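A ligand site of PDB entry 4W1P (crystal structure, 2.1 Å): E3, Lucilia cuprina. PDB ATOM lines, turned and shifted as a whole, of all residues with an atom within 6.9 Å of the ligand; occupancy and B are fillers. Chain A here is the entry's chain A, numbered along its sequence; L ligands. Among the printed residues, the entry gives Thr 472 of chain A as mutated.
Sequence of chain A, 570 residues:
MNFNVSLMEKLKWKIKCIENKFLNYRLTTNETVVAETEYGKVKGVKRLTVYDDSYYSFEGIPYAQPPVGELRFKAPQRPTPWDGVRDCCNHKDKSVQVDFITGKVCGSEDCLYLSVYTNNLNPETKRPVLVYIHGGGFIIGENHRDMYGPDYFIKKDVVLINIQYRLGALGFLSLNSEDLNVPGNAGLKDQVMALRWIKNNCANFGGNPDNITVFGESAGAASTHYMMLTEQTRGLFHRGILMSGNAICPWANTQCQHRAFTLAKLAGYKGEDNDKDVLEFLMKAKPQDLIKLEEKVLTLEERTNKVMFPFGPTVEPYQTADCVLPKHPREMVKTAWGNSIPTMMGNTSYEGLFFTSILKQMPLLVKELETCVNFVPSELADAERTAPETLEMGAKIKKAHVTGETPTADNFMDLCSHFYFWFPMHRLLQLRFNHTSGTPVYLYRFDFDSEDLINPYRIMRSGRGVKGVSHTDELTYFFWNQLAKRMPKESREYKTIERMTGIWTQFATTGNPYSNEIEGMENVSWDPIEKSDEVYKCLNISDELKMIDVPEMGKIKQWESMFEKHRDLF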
ATOM      1  N   HIS A 134     -18.007  10.970 -19.346  1.00  0.00           N
ATOM      2  CA  HIS A 134     -17.167   9.790 -19.138  1.00  0.00           C
ATOM      3  C   HIS A 134     -15.904  10.138 -18.338  1.00  0.00           C
ATOM      4  O   HIS A 134     -15.458  11.278 -18.338  1.00  0.00           O
ATOM      5  CB  HIS A 134     -16.785   9.163 -20.477  1.00  0.00           C
ATOM      6  CG  HIS A 134     -15.802   9.965 -21.262  1.00  0.00           C
ATOM      7  ND1 HIS A 134     -14.439   9.943 -21.001  1.00  0.00           N
ATOM      8  CD2 HIS A 134     -15.962  10.802 -22.314  1.00  0.00           C
ATOM      9  CE1 HIS A 134     -13.819  10.719 -21.864  1.00  0.00           C
ATOM     10  NE2 HIS A 134     -14.718  11.257 -22.670  1.00  0.00           N
ATOM     11  N   GLY A 135     -15.340   9.142 -17.651  1.00  0.00           N
ATOM     12  CA  GLY A 135     -14.066   9.307 -16.983  1.00  0.00           C
ATOM     13  C   GLY A 135     -12.969   8.811 -17.870  1.00  0.00           C
ATOM     14  O   GLY A 135     -13.180   8.621 -19.069  1.00  0.00           O
ATOM     15  N   GLY A 136     -11.791   8.571 -17.292  1.00  0.00           N
ATOM     16  CA  GLY A 136     -10.624   8.203 -18.076  1.00  0.00           C
ATOM     17  C   GLY A 136      -9.485   9.163 -17.783  1.00  0.00           C
ATOM     18  O   GLY A 136      -8.703   9.513 -18.672  1.00  0.00           O
ATOM     19  N   GLY A 137      -9.424   9.586 -16.521  1.00  0.00           N
ATOM     20  CA  GLY A 137      -8.366  10.425 -15.996  1.00  0.00           C
ATOM     21  C   GLY A 137      -8.103  11.712 -16.749  1.00  0.00           C
ATOM     22  O   GLY A 137      -7.033  12.294 -16.598  1.00  0.00           O
ATOM     23  N   PHE A 138      -9.081  12.141 -17.547  1.00  0.00           N
ATOM     24  CA  PHE A 138      -9.001  13.332 -18.403  1.00  0.00           C
ATOM     25  C   PHE A 138      -8.061  13.161 -19.597  1.00  0.00           C
ATOM     26  O   PHE A 138      -7.718  14.138 -20.273  1.00  0.00           O
ATOM     27  CB  PHE A 138      -8.570  14.571 -17.611  1.00  0.00           C
ATOM     28  CG  PHE A 138      -9.582  15.043 -16.614  1.00  0.00           C
ATOM     29  CD1 PHE A 138     -10.753  15.623 -17.016  1.00  0.00           C
ATOM     30  CD2 PHE A 138      -9.330  14.921 -15.246  1.00  0.00           C
ATOM     31  CE1 PHE A 138     -11.686  16.077 -16.091  1.00  0.00           C
ATOM     32  CE2 PHE A 138     -10.262  15.366 -14.311  1.00  0.00           C
ATOM     33  CZ  PHE A 138     -11.436  15.951 -14.736  1.00  0.00           C
ATOM     34  N   ILE A 140      -8.188   9.734 -21.542  1.00  0.00           N
ATOM     35  CA  ILE A 140      -8.809   8.772 -22.458  1.00  0.00           C
ATOM     36  C   ILE A 140     -10.316   8.833 -22.327  1.00  0.00           C
ATOM     37  O   ILE A 140     -10.828   9.477 -21.405  1.00  0.00           O
ATOM     38  CB  ILE A 140      -8.372   7.304 -22.211  1.00  0.00           C
ATOM     39  CG1 ILE A 140      -8.898   6.807 -20.860  1.00  0.00           C
ATOM     40  CG2 ILE A 140      -6.844   7.118 -22.329  1.00  0.00           C
ATOM     41  CD1 ILE A 140      -8.822   5.349 -20.689  1.00  0.00           C
ATOM     42  N   GLU A 217     -18.449   9.297 -13.828  1.00  0.00           N
ATOM     43  CA  GLU A 217     -17.683   8.354 -13.020  1.00  0.00           C
ATOM     44  C   GLU A 217     -16.166   8.653 -13.164  1.00  0.00           C
ATOM     45  O   GLU A 217     -15.730   9.031 -14.244  1.00  0.00           O
ATOM     46  CB  GLU A 217     -18.059   6.933 -13.445  1.00  0.00           C
ATOM     47  CG  GLU A 217     -17.612   5.830 -12.522  1.00  0.00           C
ATOM     48  CD  GLU A 217     -16.329   5.174 -12.994  1.00  0.00           C
ATOM     49  OE1 GLU A 217     -16.019   5.273 -14.205  1.00  0.00           O
ATOM     50  OE2 GLU A 217     -15.615   4.576 -12.166  1.00  0.00           O
ATOM     51  N   SER A 218     -15.391   8.487 -12.080  1.00  0.00           N
ATOM     52  CA  SER A 218     -13.940   8.807 -12.066  1.00  0.00           C
ATOM     53  C   SER A 218     -13.619  10.289 -12.424  1.00  0.00           C
ATOM     54  O   SER A 218     -14.056  11.224 -11.736  1.00  0.00           O
ATOM     55  CB  SER A 218     -13.190   7.850 -12.998  1.00  0.00           C
ATOM     56  OG  SER A 218     -11.786   8.034 -12.905  1.00  0.00           O
ATOM     57  N   ALA A 219     -12.863  10.503 -13.505  1.00  0.00           N
ATOM     58  CA  ALA A 219     -12.684  11.846 -14.060  1.00  0.00           C
ATOM     59  C   ALA A 219     -14.022  12.462 -14.467  1.00  0.00           C
ATOM     60  O   ALA A 219     -14.134  13.658 -14.529  1.00  0.00           O
ATOM     61  CB  ALA A 219     -11.737  11.824 -15.274  1.00  0.00           C
ATOM     62  N   GLY A 220     -14.997  11.615 -14.803  1.00  0.00           N
ATOM     63  CA  GLY A 220     -16.350  12.061 -15.105  1.00  0.00           C
ATOM     64  C   GLY A 220     -17.113  12.528 -13.888  1.00  0.00           C
ATOM     65  O   GLY A 220     -17.979  13.406 -13.983  1.00  0.00           O
ATOM     66  N   ALA A 221     -16.776  11.957 -12.734  1.00  0.00           N
ATOM     67  CA  ALA A 221     -17.344  12.402 -11.461  1.00  0.00           C
ATOM     68  C   ALA A 221     -16.751  13.756 -11.085  1.00  0.00           C
ATOM     69  O   ALA A 221     -17.484  14.689 -10.757  1.00  0.00           O
ATOM     70  CB  ALA A 221     -17.092  11.372 -10.352  1.00  0.00           C
ATOM     71  N   SER A 244     -17.724   7.664  -7.638  1.00  0.00           N
ATOM     72  CA  SER A 244     -16.291   7.407  -7.415  1.00  0.00           C
ATOM     73  C   SER A 244     -15.448   8.621  -7.801  1.00  0.00           C
ATOM     74  O   SER A 244     -14.497   8.496  -8.579  1.00  0.00           O
ATOM     75  CB  SER A 244     -15.792   6.201  -8.226  1.00  0.00           C
ATOM     76  OG  SER A 244     -16.322   4.982  -7.732  1.00  0.00           O
ATOM     77  N   TRP A 251      -6.021  13.597  -7.578  1.00  0.00           N
ATOM     78  CA  TRP A 251      -5.751  13.444  -9.009  1.00  0.00           C
ATOM     79  C   TRP A 251      -6.583  14.394  -9.896  1.00  0.00           C
ATOM     80  O   TRP A 251      -6.351  14.486 -11.103  1.00  0.00           O
ATOM     81  CB  TRP A 251      -6.043  11.998  -9.437  1.00  0.00           C
ATOM     82  CG  TRP A 251      -7.341  11.516  -8.908  1.00  0.00           C
ATOM     83  CD1 TRP A 251      -7.546  10.879  -7.727  1.00  0.00           C
ATOM     84  CD2 TRP A 251      -8.628  11.680  -9.514  1.00  0.00           C
ATOM     85  NE1 TRP A 251      -8.892  10.619  -7.557  1.00  0.00           N
ATOM     86  CE2 TRP A 251      -9.580  11.098  -8.641  1.00  0.00           C
ATOM     87  CE3 TRP A 251      -9.085  12.248 -10.708  1.00  0.00           C
ATOM     88  CZ2 TRP A 251     -10.950  11.075  -8.931  1.00  0.00           C
ATOM     89  CZ3 TRP A 251     -10.451  12.216 -10.996  1.00  0.00           C
ATOM     90  CH2 TRP A 251     -11.359  11.628 -10.101  1.00  0.00           C
ATOM     91  N   ALA A 252      -7.533  15.113  -9.313  1.00  0.00           N
ATOM     92  CA  ALA A 252      -8.544  15.822 -10.119  1.00  0.00           C
ATOM     93  C   ALA A 252      -8.203  17.273 -10.456  1.00  0.00           C
ATOM     94  O   ALA A 252      -8.961  17.958 -11.143  1.00  0.00           O
ATOM     95  CB  ALA A 252      -9.901  15.756  -9.432  1.00  0.00           C
ATOM     96  N   MET A 308      -0.603  12.172 -10.760  1.00  0.00           N
ATOM     97  CA  MET A 308      -0.991  11.060 -11.610  1.00  0.00           C
ATOM     98  C   MET A 308      -0.937  11.412 -13.106  1.00  0.00           C
ATOM     99  O   MET A 308      -0.561  10.588 -13.931  1.00  0.00           O
ATOM    100  CB  MET A 308      -2.383  10.579 -11.221  1.00  0.00           C
ATOM    101  CG  MET A 308      -2.738   9.228 -11.810  1.00  0.00           C
ATOM    102  SD  MET A 308      -4.397   8.661 -11.364  1.00  0.00           S
ATOM    103  CE  MET A 308      -4.216   8.337  -9.618  1.00  0.00           C
ATOM    104  N   PHE A 309      -1.303  12.659 -13.433  1.00  0.00           N
ATOM    105  CA  PHE A 309      -1.343  13.086 -14.826  1.00  0.00           C
ATOM    106  C   PHE A 309      -0.629  14.432 -15.021  1.00  0.00           C
ATOM    107  O   PHE A 309      -0.784  15.327 -14.200  1.00  0.00           O
ATOM    108  CB  PHE A 309      -2.789  13.193 -15.293  1.00  0.00           C
ATOM    109  CG  PHE A 309      -3.624  11.982 -14.970  1.00  0.00           C
ATOM    110  CD1 PHE A 309      -3.494  10.813 -15.711  1.00  0.00           C
ATOM    111  CD2 PHE A 309      -4.552  12.020 -13.949  1.00  0.00           C
ATOM    112  CE1 PHE A 309      -4.272   9.692 -15.431  1.00  0.00           C
ATOM    113  CE2 PHE A 309      -5.341  10.894 -13.664  1.00  0.00           C
ATOM    114  CZ  PHE A 309      -5.195   9.731 -14.419  1.00  0.00           C
ATOM    115  N   PHE A 354      -8.476  -1.786  -8.085  1.00  0.00           N
ATOM    116  CA  PHE A 354      -8.097  -1.364  -9.417  1.00  0.00           C
ATOM    117  C   PHE A 354      -6.578  -1.375  -9.674  1.00  0.00           C
ATOM    118  O   PHE A 354      -6.129  -1.677 -10.784  1.00  0.00           O
ATOM    119  CB  PHE A 354      -8.662   0.049  -9.655  1.00  0.00           C
ATOM    120  CG  PHE A 354      -8.424   0.573 -11.020  1.00  0.00           C
ATOM    121  CD1 PHE A 354      -7.287   1.295 -11.310  1.00  0.00           C
ATOM    122  CD2 PHE A 354      -9.340   0.331 -12.038  1.00  0.00           C
ATOM    123  CE1 PHE A 354      -7.055   1.776 -12.591  1.00  0.00           C
ATOM    124  CE2 PHE A 354      -9.130   0.823 -13.317  1.00  0.00           C
ATOM    125  CZ  PHE A 354      -7.973   1.538 -13.587  1.00  0.00           C
ATOM    126  N   PHE A 355      -5.786  -1.062  -8.659  1.00  0.00           N
ATOM    127  CA  PHE A 355      -4.347  -0.845  -8.828  1.00  0.00           C
ATOM    128  C   PHE A 355      -3.497  -2.096  -8.881  1.00  0.00           C
ATOM    129  O   PHE A 355      -2.265  -2.000  -8.828  1.00  0.00           O
ATOM    130  CB  PHE A 355      -3.815   0.032  -7.705  1.00  0.00           C
ATOM    131  CG  PHE A 355      -4.237   1.457  -7.811  1.00  0.00           C
ATOM    132  CD1 PHE A 355      -3.587   2.329  -8.674  1.00  0.00           C
ATOM    133  CD2 PHE A 355      -5.310   1.923  -7.072  1.00  0.00           C
ATOM    134  CE1 PHE A 355      -3.996   3.634  -8.782  1.00  0.00           C
ATOM    135  CE2 PHE A 355      -5.715   3.228  -7.189  1.00  0.00           C
ATOM    136  CZ  PHE A 355      -5.060   4.083  -8.039  1.00  0.00           C
ATOM    137  N   TYR A 420      -7.499   8.060  -2.771  1.00  0.00           N
ATOM    138  CA  TYR A 420      -8.032   8.578  -4.009  1.00  0.00           C
ATOM    139  C   TYR A 420      -9.534   8.885  -3.982  1.00  0.00           C
ATOM    140  O   TYR A 420      -9.984   9.731  -4.744  1.00  0.00           O
ATOM    141  CB  TYR A 420      -7.730   7.610  -5.165  1.00  0.00           C
ATOM    142  CG  TYR A 420      -6.258   7.525  -5.486  1.00  0.00           C
ATOM    143  CD1 TYR A 420      -5.586   8.610  -6.051  1.00  0.00           C
ATOM    144  CD2 TYR A 420      -5.541   6.358  -5.241  1.00  0.00           C
ATOM    145  CE1 TYR A 420      -4.217   8.548  -6.334  1.00  0.00           C
ATOM    146  CE2 TYR A 420      -4.186   6.285  -5.532  1.00  0.00           C
ATOM    147  CZ  TYR A 420      -3.529   7.378  -6.080  1.00  0.00           C
ATOM    148  OH  TYR A 420      -2.182   7.291  -6.365  1.00  0.00           O
ATOM    149  N   PHE A 421     -10.312   8.222  -3.114  1.00  0.00           N
ATOM    150  CA  PHE A 421     -11.783   8.355  -3.173  1.00  0.00           C
ATOM    151  C   PHE A 421     -12.506   8.682  -1.843  1.00  0.00           C
ATOM    152  O   PHE A 421     -13.193   9.694  -1.756  1.00  0.00           O
ATOM    153  CB  PHE A 421     -12.374   7.076  -3.803  1.00  0.00           C
ATOM    154  CG  PHE A 421     -11.780   6.744  -5.156  1.00  0.00           C
ATOM    155  CD1 PHE A 421     -12.181   7.434  -6.289  1.00  0.00           C
ATOM    156  CD2 PHE A 421     -10.825   5.750  -5.293  1.00  0.00           C
ATOM    157  CE1 PHE A 421     -11.626   7.149  -7.535  1.00  0.00           C
ATOM    158  CE2 PHE A 421     -10.261   5.448  -6.536  1.00  0.00           C
ATOM    159  CZ  PHE A 421     -10.666   6.165  -7.646  1.00  0.00           C
ATOM    160  N   TYR A 457     -12.606  -1.921 -18.812  1.00  0.00           N
ATOM    161  CA  TYR A 457     -11.624  -1.498 -17.814  1.00  0.00           C
ATOM    162  C   TYR A 457     -11.054  -2.684 -17.058  1.00  0.00           C
ATOM    163  O   TYR A 457      -9.971  -2.600 -16.451  1.00  0.00           O
ATOM    164  CB  TYR A 457     -12.233  -0.500 -16.827  1.00  0.00           C
ATOM    165  CG  TYR A 457     -12.349   0.912 -17.340  1.00  0.00           C
ATOM    166  CD1 TYR A 457     -11.230   1.750 -17.360  1.00  0.00           C
ATOM    167  CD2 TYR A 457     -13.565   1.414 -17.782  1.00  0.00           C
ATOM    168  CE1 TYR A 457     -11.333   3.054 -17.816  1.00  0.00           C
ATOM    169  CE2 TYR A 457     -13.675   2.703 -18.232  1.00  0.00           C
ATOM    170  CZ  TYR A 457     -12.559   3.528 -18.255  1.00  0.00           C
ATOM    171  OH  TYR A 457     -12.662   4.822 -18.701  1.00  0.00           O
ATOM    172  N   MET A 460      -7.856  -3.520 -18.725  1.00  0.00           N
ATOM    173  CA  MET A 460      -6.827  -2.572 -18.320  1.00  0.00           C
ATOM    174  C   MET A 460      -6.250  -2.884 -16.931  1.00  0.00           C
ATOM    175  O   MET A 460      -5.039  -3.022 -16.782  1.00  0.00           O
ATOM    176  CB  MET A 460      -7.398  -1.162 -18.335  1.00  0.00           C
ATOM    177  CG  MET A 460      -6.382  -0.087 -18.007  1.00  0.00           C
ATOM    178  SD  MET A 460      -7.138   1.549 -17.843  1.00  0.00           S
ATOM    179  CE  MET A 460      -7.913   1.745 -19.446  1.00  0.00           C
ATOM    180  N   HIS A 471     -13.146  -0.050  -8.607  1.00  0.00           N
ATOM    181  CA  HIS A 471     -13.420   1.168  -9.363  1.00  0.00           C
ATOM    182  C   HIS A 471     -13.743   0.785 -10.816  1.00  0.00           C
ATOM    183  O   HIS A 471     -13.003  -0.004 -11.413  1.00  0.00           O
ATOM    184  CB  HIS A 471     -12.184   2.093  -9.270  1.00  0.00           C
ATOM    185  CG  HIS A 471     -12.332   3.401  -9.977  1.00  0.00           C
ATOM    186  ND1 HIS A 471     -13.119   4.428  -9.500  1.00  0.00           N
ATOM    187  CD2 HIS A 471     -11.795   3.852 -11.133  1.00  0.00           C
ATOM    188  CE1 HIS A 471     -13.061   5.451 -10.334  1.00  0.00           C
ATOM    189  NE2 HIS A 471     -12.261   5.128 -11.341  1.00  0.00           N
ATOM    190  N   THR A 472     -14.856   1.311 -11.350  1.00  0.00           N
ATOM    191  CA  THR A 472     -15.400   1.069 -12.716  1.00  0.00           C
ATOM    192  C   THR A 472     -16.187  -0.225 -12.917  1.00  0.00           C
ATOM    193  O   THR A 472     -16.798  -0.393 -13.974  1.00  0.00           O
ATOM    194  CB  THR A 472     -14.330   1.027 -13.844  1.00  0.00           C
ATOM    195  OG1 THR A 472     -13.585  -0.196 -13.769  1.00  0.00           O
ATOM    196  CG2 THR A 472     -13.405   2.229 -13.781  1.00  0.00           C
ATOM    197  N   LEU A 475     -19.995   0.419 -13.972  1.00  0.00           N
ATOM    198  CA  LEU A 475     -20.384   0.893 -15.295  1.00  0.00           C
ATOM    199  C   LEU A 475     -21.055  -0.212 -16.101  1.00  0.00           C
ATOM    200  O   LEU A 475     -21.830   0.034 -17.021  1.00  0.00           O
ATOM    201  CB  LEU A 475     -19.167   1.408 -16.068  1.00  0.00           C
ATOM    202  CG  LEU A 475     -18.534   2.674 -15.497  1.00  0.00           C
ATOM    203  CD1 LEU A 475     -17.284   3.044 -16.275  1.00  0.00           C
ATOM    204  CD2 LEU A 475     -19.588   3.803 -15.504  1.00  0.00           C
HETATM  205  O1  LIG L   1     -11.226   8.584 -14.586  1.00  0.00           O
HETATM  206  P1  LIG L   1     -10.687   7.459 -13.729  1.00  0.00           P
HETATM  207  O2  LIG L   1      -9.222   8.004 -13.114  1.00  0.00           O
HETATM  208  C1  LIG L   1      -9.228   8.853 -12.014  1.00  0.00           C
HETATM  209  C2  LIG L   1      -8.015   8.518 -11.154  1.00  0.00           C
HETATM  210  O3  LIG L   1     -10.192   6.330 -14.830  1.00  0.00           O
HETATM  211  C3  LIG L   1     -11.041   5.285 -15.114  1.00  0.00           C
HETATM  212  C4  LIG L   1     -10.549   4.066 -14.368  1.00  0.00           C
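N of Ala 219 lies within hydrogen-bond range of O1 of the ligand (2.7 Å).
The side-chain hydroxyl (OG) of Ser 218 is covalently linked to a phosphorus (P1) of the ligand, 1.5 Å away.
The backbone NH (N) of Gly 137 lies within hydrogen-bond range of an oxygen (O1) of the ligand (2.8 Å).
An oxygen (O1) of the ligand sits at hydrogen-bond distance from the backbone NH of Gly 136, 2.8 Å away.
The indole nitrogen of Trp 251 sits at hydrogen-bond distance from the backbone carbonyl oxygen of Tyr 420, at 3.1 Å.
The side-chain hydroxyl (OG) of Ser 218 lies close to a ring nitrogen (NE2) of His 471, at 3.3 Å.
The backbone NH (N) of Gly 135 lies close to the backbone carbonyl oxygen (O) of Glu 217.
The side-chain carboxylate (OE2) of Glu 217 sits close to a ring nitrogen (NE2) of His 471, at 3.5 Å.
The backbone NH (N) of Thr 472 is in hydrogen-bond range of the side-chain carboxylate (OE2) of Glu 217.
Residues that only touch the ligand: Gly 135, Trp 251, Met 308, Phe 354, Tyr 457, His 471 and Thr 472.
Hydrophobic or aromatic side chains that line the ligand: Ala 219, Trp 251, Met 308, Phe 354, Tyr 457 and His 471.
11 residues have an atom within 4 Å of the ligand: Gly 135, Gly 136, Gly 137, Ser 218, Ala 219, Trp 251, Met 308, Phe 354, Tyr 457, His 471 and Thr 472.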
